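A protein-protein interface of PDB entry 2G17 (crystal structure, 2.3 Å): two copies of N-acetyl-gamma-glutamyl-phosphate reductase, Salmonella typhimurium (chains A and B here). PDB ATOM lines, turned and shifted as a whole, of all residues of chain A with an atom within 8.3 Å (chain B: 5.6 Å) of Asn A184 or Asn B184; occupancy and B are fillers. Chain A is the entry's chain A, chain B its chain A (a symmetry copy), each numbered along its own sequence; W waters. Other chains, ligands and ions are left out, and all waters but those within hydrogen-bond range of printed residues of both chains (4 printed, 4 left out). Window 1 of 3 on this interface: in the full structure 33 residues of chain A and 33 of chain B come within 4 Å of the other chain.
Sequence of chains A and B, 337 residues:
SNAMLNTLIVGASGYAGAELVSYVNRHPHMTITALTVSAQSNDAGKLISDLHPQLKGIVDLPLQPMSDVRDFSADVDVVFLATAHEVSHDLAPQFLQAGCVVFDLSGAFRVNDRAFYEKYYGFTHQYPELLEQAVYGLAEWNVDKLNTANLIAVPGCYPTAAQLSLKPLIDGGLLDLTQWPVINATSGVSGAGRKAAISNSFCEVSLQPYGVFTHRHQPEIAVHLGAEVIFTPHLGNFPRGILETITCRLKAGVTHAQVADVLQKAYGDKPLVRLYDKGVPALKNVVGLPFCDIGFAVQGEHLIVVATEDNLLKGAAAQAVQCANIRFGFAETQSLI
The side-chain amide nitrogen of Asn A184 lies close to the side-chain amide nitrogen of Asn B184 (2.5 Å). A ring nitrogen (NE2) of His A234 is in hydrogen-bond range of the side-chain hydroxyl (OG1) of Thr B245 (2.8 Å). A ring nitrogen (NE2) of His B234 sits at hydrogen-bond distance from the side-chain hydroxyl (OG1) of Thr A245.
The backbone carbonyl oxygen (O) of Thr A232 sits at hydrogen-bond distance from a ring nitrogen (ND1) of His A234 (3.1 Å). The backbone NH (N) of Ile B183 lies within hydrogen-bond range of the backbone carbonyl oxygen (O) of Ile B230, 2.7 Å away. The backbone carbonyl oxygen (O) of Asn B184 is in hydrogen-bond range of the backbone NH (N) of Thr B245 (2.8 Å). O of Thr B232 is in hydrogen-bond range of N of Ala B185 (3.0 Å). ND1 of His B234 is in hydrogen-bond range of O of Thr B232, at 3.1 Å.
Among the printed residues, pairs that only touch across the chains: Val A182 with Thr B247 (3.8 Å), Asn A184 with Thr B245 (3.4 Å), Leu A207 with Thr B186 (3.6 Å), Leu A207 with Leu B243 (3.4 Å), Pro A209 with Leu B243 (3.8 Å), Pro A209 with Thr B245 (3.96 Å), Thr A245 with Asn B184 (3.4 Å), Thr A247 with Val B182 (3.8 Å), Ile A304 with Ile B230 (3.9 Å) and Ile A304 with Thr B232 (3.4 Å).
Asn A184 touches just these residues of chain B: Asn B184 (2.5 Å) and Thr B245 (3.4 Å). Of chain A, only Asn A184 and Thr A245 come within 4 Å of Asn B184. Ala B185 touches none of the printed residues of chain A. Of the printed residues of chain A, Ile B230 touches Ile A304 (3.9 Å). Of the printed residues of chain A, Leu B243 touches Leu A207 and Pro A209. The nearest residue of chain B that does not touch Asn A184 is Thr B247 (4.4 Å). The nearest residue of chain A that does not touch Asn B184 is Thr A247 (4.4 Å). The nearest printed residue of chain B that does not touch Val A182 is Val B182 (4.5 Å).
Of the 26 printed residues of chain A, 8 touch a printed residue of chain B. Of the 13 printed residues of chain B, 9 touch a printed residue of chain A. Hydrophobic or aromatic side chains of chain B within 4 Å of the printed part of chain A: Val B182, Ile B230, His B234 and Leu B243. Among the printed residues, no Asp or Glu carboxylate lies within 4 Å of a Lys or Arg side-chain nitrogen of the other chain.
Val A182 touches Thr B247, and with the chains exchanged Thr A247 touches Val B182. Asn A184 touches its own counterpart, Asn B184. Asn A184 touches Thr B245, and with the chains exchanged Thr A245 touches Asn B184. His A234 touches Thr B245, and with the chains exchanged Thr A245 touches His B234. 13 positions are printed for both chains. Of the 13 pairs that touch across the chains among the printed residues, 7 have their exchanged pair printed and touching as well.
Water W3 lies within hydrogen-bond range of the backbone carbonyl oxygen of Thr A245 (2.7 Å), the side-chain amide nitrogen of Asn B184 (2.7 Å), the side-chain hydroxyl of Thr A247 (2.8 Å), the backbone carbonyl oxygen of Val A182 (3.0 Å) and the side-chain amide nitrogen of Asn A184 (3.5 Å).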
ATOM      1  N   TYR A 158      -0.118  10.759   4.656  1.00  0.00           N
ATOM      2  CA  TYR A 158      -0.261   9.776   3.597  1.00  0.00           C
ATOM      3  C   TYR A 158      -0.510   8.334   4.122  1.00  0.00           C
ATOM      4  O   TYR A 158      -1.344   7.616   3.566  1.00  0.00           O
ATOM      5  CB  TYR A 158       0.971   9.776   2.694  1.00  0.00           C
ATOM      6  CG  TYR A 158       1.241  10.997   1.797  1.00  0.00           C
ATOM      7  CD1 TYR A 158       0.451  11.250   0.656  1.00  0.00           C
ATOM      8  CD2 TYR A 158       2.397  11.792   1.989  1.00  0.00           C
ATOM      9  CE1 TYR A 158       0.770  12.310  -0.223  1.00  0.00           C
ATOM     10  CE2 TYR A 158       2.697  12.865   1.142  1.00  0.00           C
ATOM     11  CZ  TYR A 158       1.877  13.102   0.036  1.00  0.00           C
ATOM     12  OH  TYR A 158       2.201  14.113  -0.831  1.00  0.00           O
ATOM     13  N   ALA A 162      -3.629   5.474   3.199  1.00  0.00           N
ATOM     14  CA  ALA A 162      -3.059   4.230   2.661  1.00  0.00           C
ATOM     15  C   ALA A 162      -3.443   2.986   3.472  1.00  0.00           C
ATOM     16  O   ALA A 162      -3.834   1.952   2.898  1.00  0.00           O
ATOM     17  CB  ALA A 162      -1.520   4.329   2.521  1.00  0.00           C
ATOM     18  N   PRO A 181       1.235  -3.598  -3.790  1.00  0.00           N
ATOM     19  CA  PRO A 181       0.311  -2.486  -4.041  1.00  0.00           C
ATOM     20  C   PRO A 181       1.037  -1.203  -4.473  1.00  0.00           C
ATOM     21  O   PRO A 181       2.116  -0.879  -3.933  1.00  0.00           O
ATOM     22  CB  PRO A 181      -0.366  -2.289  -2.680  1.00  0.00           C
ATOM     23  CG  PRO A 181      -0.420  -3.715  -2.104  1.00  0.00           C
ATOM     24  CD  PRO A 181       0.979  -4.256  -2.485  1.00  0.00           C
ATOM     25  N   VAL A 182       0.459  -0.501  -5.453  1.00  0.00           N
ATOM     26  CA  VAL A 182       0.996   0.759  -5.910  1.00  0.00           C
ATOM     27  C   VAL A 182       0.150   1.929  -5.392  1.00  0.00           C
ATOM     28  O   VAL A 182      -0.996   2.130  -5.805  1.00  0.00           O
ATOM     29  CB  VAL A 182       1.097   0.827  -7.443  1.00  0.00           C
ATOM     30  CG1 VAL A 182       1.629   2.229  -7.900  1.00  0.00           C
ATOM     31  CG2 VAL A 182       2.000  -0.313  -7.995  1.00  0.00           C
ATOM     32  N   ILE A 183       0.749   2.727  -4.516  1.00  0.00           N
ATOM     33  CA  ILE A 183       0.069   3.873  -3.932  1.00  0.00           C
ATOM     34  C   ILE A 183       0.564   5.136  -4.595  1.00  0.00           C
ATOM     35  O   ILE A 183       1.712   5.544  -4.380  1.00  0.00           O
ATOM     36  CB  ILE A 183       0.338   3.952  -2.402  1.00  0.00           C
ATOM     37  CG1 ILE A 183       0.053   2.578  -1.764  1.00  0.00           C
ATOM     38  CG2 ILE A 183      -0.472   5.124  -1.755  1.00  0.00           C
ATOM     39  CD1 ILE A 183       0.579   2.404  -0.348  1.00  0.00           C
ATOM     40  N   ASN A 184      -0.289   5.737  -5.413  1.00  0.00           N
ATOM     41  CA  ASN A 184      -0.009   7.042  -5.994  1.00  0.00           C
ATOM     42  C   ASN A 184      -0.808   8.094  -5.259  1.00  0.00           C
ATOM     43  O   ASN A 184      -2.026   8.082  -5.263  1.00  0.00           O
ATOM     44  CB  ASN A 184      -0.326   7.096  -7.497  1.00  0.00           C
ATOM     45  CG  ASN A 184       0.827   6.552  -8.353  1.00  0.00           C
ATOM     46  OD1 ASN A 184       1.897   7.138  -8.425  1.00  0.00           O
ATOM     47  ND2 ASN A 184       0.609   5.390  -8.976  1.00  0.00           N
ATOM     48  N   ALA A 185      -0.124   9.012  -4.626  1.00  0.00           N
ATOM     49  CA  ALA A 185      -0.804   9.960  -3.756  1.00  0.00           C
ATOM     50  C   ALA A 185      -0.447  11.407  -4.125  1.00  0.00           C
ATOM     51  O   ALA A 185       0.683  11.687  -4.536  1.00  0.00           O
ATOM     52  CB  ALA A 185      -0.431   9.653  -2.313  1.00  0.00           C
ATOM     53  N   THR A 186      -1.431  12.297  -4.026  1.00  0.00           N
ATOM     54  CA  THR A 186      -1.216  13.735  -4.231  1.00  0.00           C
ATOM     55  C   THR A 186      -1.670  14.501  -3.017  1.00  0.00           C
ATOM     56  O   THR A 186      -2.787  14.286  -2.563  1.00  0.00           O
ATOM     57  CB  THR A 186      -1.974  14.273  -5.471  1.00  0.00           C
ATOM     58  OG1 THR A 186      -1.560  13.523  -6.625  1.00  0.00           O
ATOM     59  CG2 THR A 186      -1.642  15.754  -5.724  1.00  0.00           C
ATOM     60  N   SER A 187      -0.819  15.411  -2.525  1.00  0.00           N
ATOM     61  CA  SER A 187      -1.137  16.271  -1.377  1.00  0.00           C
ATOM     62  C   SER A 187      -1.190  17.743  -1.752  1.00  0.00           C
ATOM     63  O   SER A 187      -0.424  18.197  -2.592  1.00  0.00           O
ATOM     64  CB  SER A 187      -0.044  16.121  -0.296  1.00  0.00           C
ATOM     65  OG  SER A 187      -0.398  16.874   0.864  1.00  0.00           O
ATOM     66  N   LEU A 207       2.486  20.186 -10.426  1.00  0.00           N
ATOM     67  CA  LEU A 207       2.305  18.793 -10.032  1.00  0.00           C
ATOM     68  C   LEU A 207       3.649  18.143 -10.294  1.00  0.00           C
ATOM     69  O   LEU A 207       4.186  18.258 -11.398  1.00  0.00           O
ATOM     70  CB  LEU A 207       1.187  18.099 -10.879  1.00  0.00           C
ATOM     71  CG  LEU A 207       0.808  16.655 -10.477  1.00  0.00           C
ATOM     72  CD1 LEU A 207       0.452  16.536  -9.006  1.00  0.00           C
ATOM     73  CD2 LEU A 207      -0.308  16.079 -11.390  1.00  0.00           C
ATOM     74  N   PRO A 209       5.996  14.443  -8.790  1.00  0.00           N
ATOM     75  CA  PRO A 209       6.333  13.399  -7.816  1.00  0.00           C
ATOM     76  C   PRO A 209       7.578  13.813  -7.051  1.00  0.00           C
ATOM     77  O   PRO A 209       8.395  14.578  -7.585  1.00  0.00           O
ATOM     78  CB  PRO A 209       6.607  12.145  -8.680  1.00  0.00           C
ATOM     79  CG  PRO A 209       6.189  12.502 -10.073  1.00  0.00           C
ATOM     80  CD  PRO A 209       6.182  13.996 -10.188  1.00  0.00           C
ATOM     81  N   ILE A 230       4.619   0.002  -3.180  1.00  0.00           N
ATOM     82  CA  ILE A 230       5.168   1.168  -3.878  1.00  0.00           C
ATOM     83  C   ILE A 230       4.374   2.401  -3.399  1.00  0.00           C
ATOM     84  O   ILE A 230       3.138   2.392  -3.409  1.00  0.00           O
ATOM     85  CB  ILE A 230       5.112   1.060  -5.430  1.00  0.00           C
ATOM     86  CG1 ILE A 230       5.772  -0.238  -5.925  1.00  0.00           C
ATOM     87  CG2 ILE A 230       5.727   2.359  -6.121  1.00  0.00           C
ATOM     88  CD1 ILE A 230       7.291  -0.259  -5.794  1.00  0.00           C
ATOM     89  N   PHE A 231       5.096   3.432  -2.948  1.00  0.00           N
ATOM     90  CA  PHE A 231       4.493   4.675  -2.472  1.00  0.00           C
ATOM     91  C   PHE A 231       5.115   5.879  -3.187  1.00  0.00           C
ATOM     92  O   PHE A 231       6.328   6.150  -3.030  1.00  0.00           O
ATOM     93  CB  PHE A 231       4.616   4.830  -0.942  1.00  0.00           C
ATOM     94  CG  PHE A 231       4.171   6.203  -0.451  1.00  0.00           C
ATOM     95  CD1 PHE A 231       2.834   6.607  -0.593  1.00  0.00           C
ATOM     96  CD2 PHE A 231       5.105   7.115   0.078  1.00  0.00           C
ATOM     97  CE1 PHE A 231       2.430   7.890  -0.213  1.00  0.00           C
ATOM     98  CE2 PHE A 231       4.713   8.392   0.486  1.00  0.00           C
ATOM     99  CZ  PHE A 231       3.379   8.776   0.357  1.00  0.00           C
ATOM    100  N   THR A 232       4.310   6.571  -4.010  1.00  0.00           N
ATOM    101  CA  THR A 232       4.801   7.756  -4.722  1.00  0.00           C
ATOM    102  C   THR A 232       3.953   8.983  -4.425  1.00  0.00           C
ATOM    103  O   THR A 232       2.819   9.086  -4.895  1.00  0.00           O
ATOM    104  CB  THR A 232       4.948   7.507  -6.236  1.00  0.00           C
ATOM    105  OG1 THR A 232       5.679   6.287  -6.430  1.00  0.00           O
ATOM    106  CG2 THR A 232       5.705   8.635  -6.903  1.00  0.00           C
ATOM    107  N   PRO A 233       4.491   9.910  -3.595  1.00  0.00           N
ATOM    108  CA  PRO A 233       3.748  11.154  -3.303  1.00  0.00           C
ATOM    109  C   PRO A 233       3.992  12.211  -4.379  1.00  0.00           C
ATOM    110  O   PRO A 233       5.012  12.174  -5.071  1.00  0.00           O
ATOM    111  CB  PRO A 233       4.340  11.602  -1.967  1.00  0.00           C
ATOM    112  CG  PRO A 233       5.854  11.115  -2.065  1.00  0.00           C
ATOM    113  CD  PRO A 233       5.806   9.836  -2.899  1.00  0.00           C
ATOM    114  N   HIS A 234       3.063  13.159  -4.490  1.00  0.00           N
ATOM    115  CA  HIS A 234       3.081  14.211  -5.523  1.00  0.00           C
ATOM    116  C   HIS A 234       2.596  15.465  -4.836  1.00  0.00           C
ATOM    117  O   HIS A 234       1.655  15.410  -4.053  1.00  0.00           O
ATOM    118  CB  HIS A 234       2.100  13.923  -6.687  1.00  0.00           C
ATOM    119  CG  HIS A 234       2.383  12.668  -7.442  1.00  0.00           C
ATOM    120  ND1 HIS A 234       2.203  11.418  -6.895  1.00  0.00           N
ATOM    121  CD2 HIS A 234       2.806  12.465  -8.717  1.00  0.00           C
ATOM    122  CE1 HIS A 234       2.527  10.496  -7.791  1.00  0.00           C
ATOM    123  NE2 HIS A 234       2.888  11.103  -8.907  1.00  0.00           N
ATOM    124  N   ILE A 242      -5.502  15.187   0.600  1.00  0.00           N
ATOM    125  CA  ILE A 242      -4.721  14.117  -0.006  1.00  0.00           C
ATOM    126  C   ILE A 242      -5.695  13.181  -0.719  1.00  0.00           C
ATOM    127  O   ILE A 242      -6.699  12.764  -0.121  1.00  0.00           O
ATOM    128  CB  ILE A 242      -3.901  13.327   1.043  1.00  0.00           C
ATOM    129  CG1 ILE A 242      -2.666  14.137   1.479  1.00  0.00           C
ATOM    130  CG2 ILE A 242      -3.466  11.978   0.492  1.00  0.00           C
ATOM    131  CD1 ILE A 242      -1.900  13.578   2.655  1.00  0.00           C
ATOM    132  N   LEU A 243      -5.400  12.858  -1.979  1.00  0.00           N
ATOM    133  CA  LEU A 243      -6.107  11.774  -2.666  1.00  0.00           C
ATOM    134  C   LEU A 243      -5.080  10.681  -2.991  1.00  0.00           C
ATOM    135  O   LEU A 243      -4.005  10.976  -3.497  1.00  0.00           O
ATOM    136  CB  LEU A 243      -6.799  12.267  -3.955  1.00  0.00           C
ATOM    137  CG  LEU A 243      -7.630  11.229  -4.732  1.00  0.00           C
ATOM    138  CD1 LEU A 243      -8.863  11.881  -5.367  1.00  0.00           C
ATOM    139  CD2 LEU A 243      -6.786  10.482  -5.800  1.00  0.00           C
ATOM    140  N   GLU A 244      -5.413   9.424  -2.703  1.00  0.00           N
ATOM    141  CA  GLU A 244      -4.546   8.305  -3.081  1.00  0.00           C
ATOM    142  C   GLU A 244      -5.294   7.379  -3.989  1.00  0.00           C
ATOM    143  O   GLU A 244      -6.452   7.021  -3.702  1.00  0.00           O
ATOM    144  CB  GLU A 244      -4.074   7.552  -1.828  1.00  0.00           C
ATOM    145  CG  GLU A 244      -3.577   8.480  -0.718  1.00  0.00           C
ATOM    146  CD  GLU A 244      -2.858   7.776   0.424  1.00  0.00           C
ATOM    147  OE1 GLU A 244      -2.820   6.536   0.461  1.00  0.00           O
ATOM    148  OE2 GLU A 244      -2.337   8.474   1.312  1.00  0.00           O
ATOM    149  N   THR A 245      -4.632   6.970  -5.076  1.00  0.00           N
ATOM    150  CA  THR A 245      -5.153   5.954  -5.982  1.00  0.00           C
ATOM    151  C   THR A 245      -4.284   4.705  -5.824  1.00  0.00           C
ATOM    152  O   THR A 245      -3.064   4.697  -6.122  1.00  0.00           O
ATOM    153  CB  THR A 245      -5.168   6.458  -7.431  1.00  0.00           C
ATOM    154  OG1 THR A 245      -5.952   7.660  -7.503  1.00  0.00           O
ATOM    155  CG2 THR A 245      -5.760   5.421  -8.408  1.00  0.00           C
ATOM    156  N   ILE A 246      -4.904   3.636  -5.339  1.00  0.00           N
ATOM    157  CA  ILE A 246      -4.146   2.467  -4.942  1.00  0.00           C
ATOM    158  C   ILE A 246      -4.526   1.273  -5.803  1.00  0.00           C
ATOM    159  O   ILE A 246      -5.672   0.828  -5.786  1.00  0.00           O
ATOM    160  CB  ILE A 246      -4.347   2.172  -3.422  1.00  0.00           C
ATOM    161  CG1 ILE A 246      -4.033   3.450  -2.612  1.00  0.00           C
ATOM    162  CG2 ILE A 246      -3.504   0.984  -3.007  1.00  0.00           C
ATOM    163  CD1 ILE A 246      -4.299   3.341  -1.106  1.00  0.00           C
ATOM    164  N   THR A 247      -3.546   0.754  -6.543  1.00  0.00           N
ATOM    165  CA  THR A 247      -3.777  -0.290  -7.526  1.00  0.00           C
ATOM    166  C   THR A 247      -3.177  -1.600  -7.036  1.00  0.00           C
ATOM    167  O   THR A 247      -1.983  -1.646  -6.676  1.00  0.00           O
ATOM    168  CB  THR A 247      -3.199   0.126  -8.900  1.00  0.00           C
ATOM    169  OG1 THR A 247      -3.786   1.386  -9.263  1.00  0.00           O
ATOM    170  CG2 THR A 247      -3.507  -0.936  -9.991  1.00  0.00           C
ATOM    171  N   ILE A 304      -8.703  -1.201  -7.882  1.00  0.00           N
ATOM    172  CA  ILE A 304      -8.298   0.163  -7.607  1.00  0.00           C
ATOM    173  C   ILE A 304      -9.117   0.699  -6.417  1.00  0.00           C
ATOM    174  O   ILE A 304     -10.345   0.713  -6.462  1.00  0.00           O
ATOM    175  CB  ILE A 304      -8.458   1.055  -8.865  1.00  0.00           C
ATOM    176  CG1 ILE A 304      -7.544   0.539 -10.008  1.00  0.00           C
ATOM    177  CG2 ILE A 304      -8.189   2.555  -8.565  1.00  0.00           C
ATOM    178  CD1 ILE A 304      -7.904   1.116 -11.387  1.00  0.00           C
ATOM    179  N   VAL A 305      -8.434   1.102  -5.352  1.00  0.00           N
ATOM    180  CA  VAL A 305      -9.052   1.789  -4.216  1.00  0.00           C
ATOM    181  C   VAL A 305      -8.671   3.262  -4.275  1.00  0.00           C
ATOM    182  O   VAL A 305      -7.507   3.601  -4.527  1.00  0.00           O
ATOM    183  CB  VAL A 305      -8.592   1.193  -2.840  1.00  0.00           C
ATOM    184  CG1 VAL A 305      -9.255   1.949  -1.631  1.00  0.00           C
ATOM    185  CG2 VAL A 305      -8.859  -0.295  -2.791  1.00  0.00           C
ATOM    186  N   VAL A 306      -9.661   4.140  -4.086  1.00  0.00           N
ATOM    187  CA  VAL A 306      -9.411   5.582  -4.041  1.00  0.00           C
ATOM    188  C   VAL A 306      -9.810   6.113  -2.654  1.00  0.00           C
ATOM    189  O   VAL A 306     -10.970   5.958  -2.226  1.00  0.00           O
ATOM    190  CB  VAL A 306     -10.179   6.324  -5.165  1.00  0.00           C
ATOM    191  CG1 VAL A 306      -9.974   7.857  -5.086  1.00  0.00           C
ATOM    192  CG2 VAL A 306      -9.768   5.762  -6.547  1.00  0.00           C
ATOM    193  N   ALA A 307      -8.849   6.721  -1.960  1.00  0.00           N
ATOM    194  CA  ALA A 307      -9.084   7.281  -0.611  1.00  0.00           C
ATOM    195  C   ALA A 307      -8.716   8.767  -0.543  1.00  0.00           C
ATOM    196  O   ALA A 307      -7.716   9.185  -1.108  1.00  0.00           O
ATOM    197  CB  ALA A 307      -8.315   6.479   0.448  1.00  0.00           C
ATOM    198  N   VAL B 182       1.205   0.161 -14.449  1.00  0.00           N
ATOM    199  CA  VAL B 182       0.177   0.997 -13.878  1.00  0.00           C
ATOM    200  C   VAL B 182       0.403   2.467 -14.254  1.00  0.00           C
ATOM    201  O   VAL B 182       1.351   3.112 -13.795  1.00  0.00           O
ATOM    202  CB  VAL B 182       0.093   0.857 -12.349  1.00  0.00           C
ATOM    203  CG1 VAL B 182      -0.995   1.822 -11.765  1.00  0.00           C
ATOM    204  CG2 VAL B 182      -0.197  -0.615 -11.939  1.00  0.00           C
ATOM    205  N   ILE B 183      -0.507   3.002 -15.058  1.00  0.00           N
ATOM    206  CA  ILE B 183      -0.421   4.383 -15.505  1.00  0.00           C
ATOM    207  C   ILE B 183      -1.409   5.220 -14.728  1.00  0.00           C
ATOM    208  O   ILE B 183      -2.624   5.096 -14.928  1.00  0.00           O
ATOM    209  CB  ILE B 183      -0.733   4.491 -17.025  1.00  0.00           C
ATOM    210  CG1 ILE B 183       0.115   3.459 -17.793  1.00  0.00           C
ATOM    211  CG2 ILE B 183      -0.545   5.959 -17.529  1.00  0.00           C
ATOM    212  CD1 ILE B 183      -0.313   3.215 -19.232  1.00  0.00           C
ATOM    213  N   ASN B 184      -0.893   6.050 -13.833  1.00  0.00           N
ATOM    214  CA  ASN B 184      -1.709   7.029 -13.129  1.00  0.00           C
ATOM    215  C   ASN B 184      -1.477   8.395 -13.734  1.00  0.00           C
ATOM    216  O   ASN B 184      -0.380   8.924 -13.701  1.00  0.00           O
ATOM    217  CB  ASN B 184      -1.412   7.064 -11.621  1.00  0.00           C
ATOM    218  CG  ASN B 184      -2.183   5.980 -10.853  1.00  0.00           C
ATOM    219  OD1 ASN B 184      -3.400   6.020 -10.747  1.00  0.00           O
ATOM    220  ND2 ASN B 184      -1.457   4.979 -10.347  1.00  0.00           N
ATOM    221  N   ALA B 185      -2.512   8.974 -14.285  1.00  0.00           N
ATOM    222  CA  ALA B 185      -2.344  10.209 -15.037  1.00  0.00           C
ATOM    223  C   ALA B 185      -3.297  11.300 -14.532  1.00  0.00           C
ATOM    224  O   ALA B 185      -4.424  11.006 -14.120  1.00  0.00           O
ATOM    225  CB  ALA B 185      -2.577   9.917 -16.512  1.00  0.00           C
ATOM    226  N   THR B 186      -2.813  12.539 -14.515  1.00  0.00           N
ATOM    227  CA  THR B 186      -3.639  13.704 -14.169  1.00  0.00           C
ATOM    228  C   THR B 186      -3.601  14.711 -15.287  1.00  0.00           C
ATOM    229  O   THR B 186      -2.516  15.061 -15.734  1.00  0.00           O
ATOM    230  CB  THR B 186      -3.169  14.392 -12.863  1.00  0.00           C
ATOM    231  OG1 THR B 186      -3.179  13.423 -11.802  1.00  0.00           O
ATOM    232  CG2 THR B 186      -4.118  15.537 -12.468  1.00  0.00           C
ATOM    233  N   ILE B 230      -2.798  -1.005 -16.758  1.00  0.00           N
ATOM    234  CA  ILE B 230      -3.791  -0.282 -15.957  1.00  0.00           C
ATOM    235  C   ILE B 230      -3.639   1.217 -16.289  1.00  0.00           C
ATOM    236  O   ILE B 230      -2.526   1.757 -16.251  1.00  0.00           O
ATOM    237  CB  ILE B 230      -3.655  -0.512 -14.424  1.00  0.00           C
ATOM    238  CG1 ILE B 230      -3.659  -2.011 -14.080  1.00  0.00           C
ATOM    239  CG2 ILE B 230      -4.766   0.301 -13.618  1.00  0.00           C
ATOM    240  CD1 ILE B 230      -5.014  -2.690 -14.249  1.00  0.00           C
ATOM    241  N   THR B 232      -5.416   4.896 -15.253  1.00  0.00           N
ATOM    242  CA  THR B 232      -6.364   5.660 -14.437  1.00  0.00           C
ATOM    243  C   THR B 232      -6.157   7.159 -14.586  1.00  0.00           C
ATOM    244  O   THR B 232      -5.174   7.706 -14.081  1.00  0.00           O
ATOM    245  CB  THR B 232      -6.350   5.219 -12.960  1.00  0.00           C
ATOM    246  OG1 THR B 232      -6.458   3.789 -12.909  1.00  0.00           O
ATOM    247  CG2 THR B 232      -7.512   5.819 -12.199  1.00  0.00           C
ATOM    248  N   HIS B 234      -7.211  11.265 -14.073  1.00  0.00           N
ATOM    249  CA  HIS B 234      -7.668  12.089 -12.939  1.00  0.00           C
ATOM    250  C   HIS B 234      -7.807  13.491 -13.482  1.00  0.00           C
ATOM    251  O   HIS B 234      -6.958  13.939 -14.244  1.00  0.00           O
ATOM    252  CB  HIS B 234      -6.634  12.149 -11.787  1.00  0.00           C
ATOM    253  CG  HIS B 234      -6.313  10.828 -11.172  1.00  0.00           C
ATOM    254  ND1 HIS B 234      -5.610   9.852 -11.838  1.00  0.00           N
ATOM    255  CD2 HIS B 234      -6.571  10.330  -9.934  1.00  0.00           C
ATOM    256  CE1 HIS B 234      -5.469   8.795 -11.050  1.00  0.00           C
ATOM    257  NE2 HIS B 234      -6.036   9.062  -9.887  1.00  0.00           N
ATOM    258  N   LEU B 243       0.445  15.009 -16.398  1.00  0.00           N
ATOM    259  CA  LEU B 243       1.576  14.287 -15.809  1.00  0.00           C
ATOM    260  C   LEU B 243       1.149  12.825 -15.622  1.00  0.00           C
ATOM    261  O   LEU B 243       0.066  12.559 -15.114  1.00  0.00           O
ATOM    262  CB  LEU B 243       2.008  14.902 -14.460  1.00  0.00           C
ATOM    263  CG  LEU B 243       3.231  14.266 -13.773  1.00  0.00           C
ATOM    264  CD1 LEU B 243       4.062  15.329 -13.046  1.00  0.00           C
ATOM    265  CD2 LEU B 243       2.833  13.118 -12.809  1.00  0.00           C
ATOM    266  N   GLU B 244       1.997  11.883 -16.028  1.00  0.00           N
ATOM    267  CA  GLU B 244       1.727  10.464 -15.789  1.00  0.00           C
ATOM    268  C   GLU B 244       2.829   9.878 -14.962  1.00  0.00           C
ATOM    269  O   GLU B 244       4.018  10.103 -15.256  1.00  0.00           O
ATOM    270  CB  GLU B 244       1.607   9.712 -17.123  1.00  0.00           C
ATOM    271  CG  GLU B 244       0.724  10.431 -18.143  1.00  0.00           C
ATOM    272  CD  GLU B 244       0.364   9.602 -19.368  1.00  0.00           C
ATOM    273  OE1 GLU B 244       0.881   8.485 -19.533  1.00  0.00           O
ATOM    274  OE2 GLU B 244      -0.432  10.084 -20.193  1.00  0.00           O
ATOM    275  N   THR B 245       2.443   9.110 -13.938  1.00  0.00           N
ATOM    276  CA  THR B 245       3.383   8.343 -13.129  1.00  0.00           C
ATOM    277  C   THR B 245       3.155   6.862 -13.434  1.00  0.00           C
ATOM    278  O   THR B 245       2.073   6.283 -13.169  1.00  0.00           O
ATOM    279  CB  THR B 245       3.207   8.650 -11.635  1.00  0.00           C
ATOM    280  OG1 THR B 245       3.378  10.062 -11.423  1.00  0.00           O
ATOM    281  CG2 THR B 245       4.220   7.890 -10.756  1.00  0.00           C
ATOM    282  N   ILE B 246       4.172   6.235 -14.010  1.00  0.00           N
ATOM    283  CA  ILE B 246       4.002   4.898 -14.544  1.00  0.00           C
ATOM    284  C   ILE B 246       4.893   3.916 -13.799  1.00  0.00           C
ATOM    285  O   ILE B 246       6.117   4.030 -13.835  1.00  0.00           O
ATOM    286  CB  ILE B 246       4.277   4.880 -16.080  1.00  0.00           C
ATOM    287  CG1 ILE B 246       3.409   5.961 -16.762  1.00  0.00           C
ATOM    288  CG2 ILE B 246       4.039   3.491 -16.634  1.00  0.00           C
ATOM    289  CD1 ILE B 246       3.660   6.136 -18.265  1.00  0.00           C
ATOM    290  N   THR B 247       4.263   2.944 -13.141  1.00  0.00           N
ATOM    291  CA  THR B 247       4.957   2.016 -12.264  1.00  0.00           C
ATOM    292  C   THR B 247       4.990   0.634 -12.900  1.00  0.00           C
ATOM    293  O   THR B 247       3.932   0.100 -13.292  1.00  0.00           O
ATOM    294  CB  THR B 247       4.288   1.990 -10.869  1.00  0.00           C
ATOM    295  OG1 THR B 247       4.263   3.335 -10.365  1.00  0.00           O
ATOM    296  CG2 THR B 247       5.061   1.070  -9.885  1.00  0.00           C
HETATM  297  O   HOH W   1      -4.398   3.204 -11.374  1.00  0.00           O
HETATM  298  O   HOH W   2       1.866   4.445 -11.204  1.00  0.00           O
HETATM  299  O   HOH W   3      -2.111   3.352  -8.258  1.00  0.00           O
HETATM  300  O   HOH W   4       4.056   5.009  -8.065  1.00  0.00           O
